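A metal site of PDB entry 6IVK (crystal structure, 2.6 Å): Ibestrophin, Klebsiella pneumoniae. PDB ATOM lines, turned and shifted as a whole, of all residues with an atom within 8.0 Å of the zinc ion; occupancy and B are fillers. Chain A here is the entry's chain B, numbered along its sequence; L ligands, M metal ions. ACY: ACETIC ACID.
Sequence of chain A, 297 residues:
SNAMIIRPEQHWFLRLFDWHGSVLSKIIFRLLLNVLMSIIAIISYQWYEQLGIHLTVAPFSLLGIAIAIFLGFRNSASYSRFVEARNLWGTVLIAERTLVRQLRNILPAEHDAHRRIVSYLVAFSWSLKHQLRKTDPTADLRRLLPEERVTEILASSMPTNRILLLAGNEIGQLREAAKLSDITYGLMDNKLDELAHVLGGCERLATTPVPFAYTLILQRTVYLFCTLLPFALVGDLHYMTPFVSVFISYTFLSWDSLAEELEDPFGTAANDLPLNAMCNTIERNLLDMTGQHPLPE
O of Glu 110 lies close to NE2 of His 114 (3.5 Å). O of Leu 103 is in hydrogen-bond range of NE2 of His 114 (3.4 Å). The backbone carbonyl oxygen (O) of Leu 107 is in hydrogen-bond range of a ring nitrogen (NE2) of His 114.
Of the 19 residues printed, 3 come within 4 Å of the zinc ion.
The zinc ion is bound by a ring nitrogen (NE2) of His 293 (1.9 Å). ND1 of His 114 binds the zinc ion, 1.9 Å away. ND1 of His 111 is bound to the zinc ion, 2.2 Å away. The zinc ion is bound by OXT of the ligand, at 2.2 Å. The zinc ion has four donor atoms within binding distance.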
ATOM      1  N   VAL A 100     -20.037  28.383 -26.211  1.00  0.00           N
ATOM      2  CA  VAL A 100     -19.434  27.265 -26.933  1.00  0.00           C
ATOM      3  C   VAL A 100     -17.946  27.529 -27.143  1.00  0.00           C
ATOM      4  O   VAL A 100     -17.134  26.614 -27.035  1.00  0.00           O
ATOM      5  CB  VAL A 100     -20.185  27.012 -28.251  1.00  0.00           C
ATOM      6  CG1 VAL A 100     -19.454  26.065 -29.190  1.00  0.00           C
ATOM      7  CG2 VAL A 100     -21.605  26.535 -28.000  1.00  0.00           C
ATOM      8  N   LEU A 103     -16.109  26.884 -23.909  1.00  0.00           N
ATOM      9  CA  LEU A 103     -16.005  25.445 -23.682  1.00  0.00           C
ATOM     10  C   LEU A 103     -14.917  24.848 -24.564  1.00  0.00           C
ATOM     11  O   LEU A 103     -14.065  24.117 -24.055  1.00  0.00           O
ATOM     12  CB  LEU A 103     -17.362  24.742 -23.895  1.00  0.00           C
ATOM     13  CG  LEU A 103     -18.421  24.976 -22.819  1.00  0.00           C
ATOM     14  CD1 LEU A 103     -19.806  24.664 -23.377  1.00  0.00           C
ATOM     15  CD2 LEU A 103     -18.141  24.190 -21.548  1.00  0.00           C
ATOM     16  N   ARG A 104     -14.916  25.202 -25.861  1.00  0.00           N
ATOM     17  CA  ARG A 104     -13.873  24.750 -26.784  1.00  0.00           C
ATOM     18  C   ARG A 104     -12.499  25.245 -26.347  1.00  0.00           C
ATOM     19  O   ARG A 104     -11.517  24.531 -26.507  1.00  0.00           O
ATOM     20  CB  ARG A 104     -14.177  25.096 -28.253  1.00  0.00           C
ATOM     21  CG  ARG A 104     -15.254  24.243 -28.912  1.00  0.00           C
ATOM     22  CD  ARG A 104     -15.960  24.806 -30.131  1.00  0.00           C
ATOM     23  NE  ARG A 104     -16.914  23.848 -30.716  1.00  0.00           N
ATOM     24  CZ  ARG A 104     -17.698  24.064 -31.794  1.00  0.00           C
ATOM     25  NH1 ARG A 104     -18.503  23.104 -32.228  1.00  0.00           N
ATOM     26  NH2 ARG A 104     -17.702  25.233 -32.412  1.00  0.00           N
ATOM     27  N   LEU A 107     -11.860  23.766 -22.270  1.00  0.00           N
ATOM     28  CA  LEU A 107     -11.974  22.318 -22.136  1.00  0.00           C
ATOM     29  C   LEU A 107     -11.965  21.706 -23.531  1.00  0.00           C
ATOM     30  O   LEU A 107     -12.929  21.036 -23.925  1.00  0.00           O
ATOM     31  CB  LEU A 107     -13.267  21.999 -21.385  1.00  0.00           C
ATOM     32  CG  LEU A 107     -13.300  22.413 -19.908  1.00  0.00           C
ATOM     33  CD1 LEU A 107     -14.655  22.141 -19.283  1.00  0.00           C
ATOM     34  CD2 LEU A 107     -12.182  21.726 -19.122  1.00  0.00           C
ATOM     35  N   PRO A 108     -10.902  21.910 -24.334  1.00  0.00           N
ATOM     36  CA  PRO A 108     -10.901  21.520 -25.752  1.00  0.00           C
ATOM     37  C   PRO A 108     -11.258  20.076 -26.050  1.00  0.00           C
ATOM     38  O   PRO A 108     -11.719  19.771 -27.147  1.00  0.00           O
ATOM     39  CB  PRO A 108      -9.465  21.805 -26.216  1.00  0.00           C
ATOM     40  CG  PRO A 108      -8.652  21.993 -24.941  1.00  0.00           C
ATOM     41  CD  PRO A 108      -9.636  22.561 -23.942  1.00  0.00           C
ATOM     42  N   ALA A 109     -11.036  19.193 -25.073  1.00  0.00           N
ATOM     43  CA  ALA A 109     -11.099  17.756 -25.270  1.00  0.00           C
ATOM     44  C   ALA A 109     -12.466  17.201 -24.875  1.00  0.00           C
ATOM     45  O   ALA A 109     -12.797  16.083 -25.269  1.00  0.00           O
ATOM     46  CB  ALA A 109      -9.993  17.075 -24.490  1.00  0.00           C
ATOM     47  N   GLU A 110     -13.259  17.977 -24.144  1.00  0.00           N
ATOM     48  CA  GLU A 110     -14.484  17.507 -23.517  1.00  0.00           C
ATOM     49  C   GLU A 110     -15.688  17.558 -24.482  1.00  0.00           C
ATOM     50  O   GLU A 110     -16.699  18.193 -24.173  1.00  0.00           O
ATOM     51  CB  GLU A 110     -14.752  18.389 -22.304  1.00  0.00           C
ATOM     52  CG  GLU A 110     -13.729  18.198 -21.211  1.00  0.00           C
ATOM     53  CD  GLU A 110     -13.867  16.928 -20.387  1.00  0.00           C
ATOM     54  OE1 GLU A 110     -14.990  16.334 -20.359  1.00  0.00           O
ATOM     55  OE2 GLU A 110     -12.856  16.532 -19.777  1.00  0.00           O
ATOM     56  N   HIS A 111     -15.602  16.834 -25.603  1.00  0.00           N
ATOM     57  CA  HIS A 111     -16.629  16.857 -26.634  1.00  0.00           C
ATOM     58  C   HIS A 111     -17.979  16.357 -26.135  1.00  0.00           C
ATOM     59  O   HIS A 111     -19.029  16.773 -26.639  1.00  0.00           O
ATOM     60  CB  HIS A 111     -16.156  16.138 -27.905  1.00  0.00           C
ATOM     61  CG  HIS A 111     -14.810  16.570 -28.387  1.00  0.00           C
ATOM     62  ND1 HIS A 111     -14.568  17.831 -28.924  1.00  0.00           N
ATOM     63  CD2 HIS A 111     -13.624  15.920 -28.416  1.00  0.00           C
ATOM     64  CE1 HIS A 111     -13.295  17.933 -29.255  1.00  0.00           C
ATOM     65  NE2 HIS A 111     -12.689  16.773 -28.950  1.00  0.00           N
ATOM     66  N   ASP A 112     -17.996  15.490 -25.121  1.00  0.00           N
ATOM     67  CA  ASP A 112     -19.270  14.958 -24.670  1.00  0.00           C
ATOM     68  C   ASP A 112     -20.092  16.086 -24.054  1.00  0.00           C
ATOM     69  O   ASP A 112     -21.294  16.204 -24.297  1.00  0.00           O
ATOM     70  CB  ASP A 112     -19.109  13.701 -23.802  1.00  0.00           C
ATOM     71  CG  ASP A 112     -18.532  12.513 -24.576  1.00  0.00           C
ATOM     72  OD1 ASP A 112     -19.107  12.156 -25.647  1.00  0.00           O
ATOM     73  OD2 ASP A 112     -17.507  11.960 -24.132  1.00  0.00           O
ATOM     74  N   ALA A 113     -19.407  16.917 -23.255  1.00  0.00           N
ATOM     75  CA  ALA A 113     -20.021  18.066 -22.620  1.00  0.00           C
ATOM     76  C   ALA A 113     -20.332  19.115 -23.689  1.00  0.00           C
ATOM     77  O   ALA A 113     -21.432  19.660 -23.711  1.00  0.00           O
ATOM     78  CB  ALA A 113     -19.130  18.580 -21.512  1.00  0.00           C
ATOM     79  N   HIS A 114     -19.394  19.316 -24.625  1.00  0.00           N
ATOM     80  CA  HIS A 114     -19.649  20.236 -25.729  1.00  0.00           C
ATOM     81  C   HIS A 114     -21.004  19.938 -26.369  1.00  0.00           C
ATOM     82  O   HIS A 114     -21.786  20.866 -26.595  1.00  0.00           O
ATOM     83  CB  HIS A 114     -18.541  20.183 -26.794  1.00  0.00           C
ATOM     84  CG  HIS A 114     -17.185  20.563 -26.294  1.00  0.00           C
ATOM     85  ND1 HIS A 114     -16.036  20.247 -26.994  1.00  0.00           N
ATOM     86  CD2 HIS A 114     -16.795  21.189 -25.155  1.00  0.00           C
ATOM     87  CE1 HIS A 114     -14.987  20.690 -26.317  1.00  0.00           C
ATOM     88  NE2 HIS A 114     -15.432  21.268 -25.169  1.00  0.00           N
ATOM     89  N   ARG A 115     -21.247  18.648 -26.639  1.00  0.00           N
ATOM     90  CA  ARG A 115     -22.411  18.145 -27.356  1.00  0.00           C
ATOM     91  C   ARG A 115     -23.641  18.287 -26.462  1.00  0.00           C
ATOM     92  O   ARG A 115     -24.685  18.797 -26.882  1.00  0.00           O
ATOM     93  CB  ARG A 115     -22.158  16.683 -27.719  1.00  0.00           C
ATOM     94  CG  ARG A 115     -23.125  16.018 -28.692  1.00  0.00           C
ATOM     95  CD  ARG A 115     -22.945  14.498 -28.776  1.00  0.00           C
ATOM     96  NE  ARG A 115     -21.728  13.879 -28.220  1.00  0.00           N
ATOM     97  CZ  ARG A 115     -20.510  13.788 -28.787  1.00  0.00           C
ATOM     98  NH1 ARG A 115     -20.259  14.310 -29.990  1.00  0.00           N
ATOM     99  NH2 ARG A 115     -19.527  13.191 -28.145  1.00  0.00           N
ATOM    100  N   VAL A 118     -24.410  22.170 -26.108  1.00  0.00           N
ATOM    101  CA  VAL A 118     -24.895  22.719 -27.358  1.00  0.00           C
ATOM    102  C   VAL A 118     -26.355  22.342 -27.603  1.00  0.00           C
ATOM    103  O   VAL A 118     -27.125  23.132 -28.152  1.00  0.00           O
ATOM    104  CB  VAL A 118     -24.010  22.320 -28.553  1.00  0.00           C
ATOM    105  CG1 VAL A 118     -24.799  22.372 -29.859  1.00  0.00           C
ATOM    106  CG2 VAL A 118     -22.784  23.219 -28.622  1.00  0.00           C
ATOM    107  N   THR A 290     -20.630  19.129 -38.028  1.00  0.00           N
ATOM    108  CA  THR A 290     -20.901  18.060 -37.069  1.00  0.00           C
ATOM    109  C   THR A 290     -20.254  18.395 -35.712  1.00  0.00           C
ATOM    110  O   THR A 290     -19.881  17.490 -34.962  1.00  0.00           O
ATOM    111  CB  THR A 290     -20.612  16.647 -37.615  1.00  0.00           C
ATOM    112  OG1 THR A 290     -19.209  16.378 -37.548  1.00  0.00           O
ATOM    113  CG2 THR A 290     -21.097  16.396 -39.035  1.00  0.00           C
ATOM    114  N   GLY A 291     -20.093  19.698 -35.441  1.00  0.00           N
ATOM    115  CA  GLY A 291     -19.681  20.196 -34.136  1.00  0.00           C
ATOM    116  C   GLY A 291     -18.175  20.132 -33.920  1.00  0.00           C
ATOM    117  O   GLY A 291     -17.724  20.286 -32.787  1.00  0.00           O
ATOM    118  N   GLN A 292     -17.405  19.957 -35.007  1.00  0.00           N
ATOM    119  CA  GLN A 292     -15.963  19.764 -34.947  1.00  0.00           C
ATOM    120  C   GLN A 292     -15.223  21.105 -34.942  1.00  0.00           C
ATOM    121  O   GLN A 292     -15.635  22.063 -35.600  1.00  0.00           O
ATOM    122  CB  GLN A 292     -15.492  18.893 -36.123  1.00  0.00           C
ATOM    123  CG  GLN A 292     -15.838  17.412 -35.975  1.00  0.00           C
ATOM    124  CD  GLN A 292     -15.424  16.626 -37.203  1.00  0.00           C
ATOM    125  OE1 GLN A 292     -14.480  16.992 -37.912  1.00  0.00           O
ATOM    126  NE2 GLN A 292     -16.134  15.554 -37.477  1.00  0.00           N
ATOM    127  N   HIS A 293     -14.088  21.145 -34.218  1.00  0.00           N
ATOM    128  CA  HIS A 293     -13.340  22.378 -33.993  1.00  0.00           C
ATOM    129  C   HIS A 293     -11.836  22.116 -34.052  1.00  0.00           C
ATOM    130  O   HIS A 293     -11.380  21.046 -33.657  1.00  0.00           O
ATOM    131  CB  HIS A 293     -13.793  23.064 -32.676  1.00  0.00           C
ATOM    132  CG  HIS A 293     -14.011  22.154 -31.503  1.00  0.00           C
ATOM    133  ND1 HIS A 293     -13.106  22.053 -30.460  1.00  0.00           N
ATOM    134  CD2 HIS A 293     -15.043  21.322 -31.201  1.00  0.00           C
ATOM    135  CE1 HIS A 293     -13.562  21.182 -29.577  1.00  0.00           C
ATOM    136  NE2 HIS A 293     -14.752  20.713 -30.011  1.00  0.00           N
ATOM    137  N   PRO A 294     -11.004  23.065 -34.551  1.00  0.00           N
ATOM    138  CA  PRO A 294      -9.560  23.013 -34.304  1.00  0.00           C
ATOM    139  C   PRO A 294      -9.282  23.028 -32.801  1.00  0.00           C
ATOM    140  O   PRO A 294     -10.008  23.677 -32.032  1.00  0.00           O
ATOM    141  CB  PRO A 294      -8.990  24.278 -34.978  1.00  0.00           C
ATOM    142  CG  PRO A 294     -10.069  24.728 -35.952  1.00  0.00           C
ATOM    143  CD  PRO A 294     -11.389  24.206 -35.412  1.00  0.00           C
ATOM    144  N   LEU A 295      -8.243  22.275 -32.393  1.00  0.00           N
ATOM    145  CA  LEU A 295      -7.880  22.134 -30.997  1.00  0.00           C
ATOM    146  C   LEU A 295      -6.567  22.854 -30.727  1.00  0.00           C
ATOM    147  O   LEU A 295      -5.653  22.778 -31.548  1.00  0.00           O
ATOM    148  CB  LEU A 295      -7.799  20.640 -30.643  1.00  0.00           C
ATOM    149  CG  LEU A 295      -9.069  20.029 -30.038  1.00  0.00           C
ATOM    150  CD1 LEU A 295      -9.989  19.453 -31.108  1.00  0.00           C
ATOM    151  CD2 LEU A 295      -8.710  18.952 -29.009  1.00  0.00           C
HETATM  152  C   ACY L   1     -18.494  19.526 -30.068  1.00  0.00           C
HETATM  153  O   ACY L   1     -18.278  20.774 -29.978  1.00  0.00           O
HETATM  154  OXT ACY L   1     -17.562  18.730 -29.715  1.00  0.00           O
HETATM  155  CH3 ACY L   1     -19.855  18.989 -30.584  1.00  0.00           C
HETATM  156 ZN    ZN M   1     -15.790  19.597 -28.814  1.00  0.00          ZN
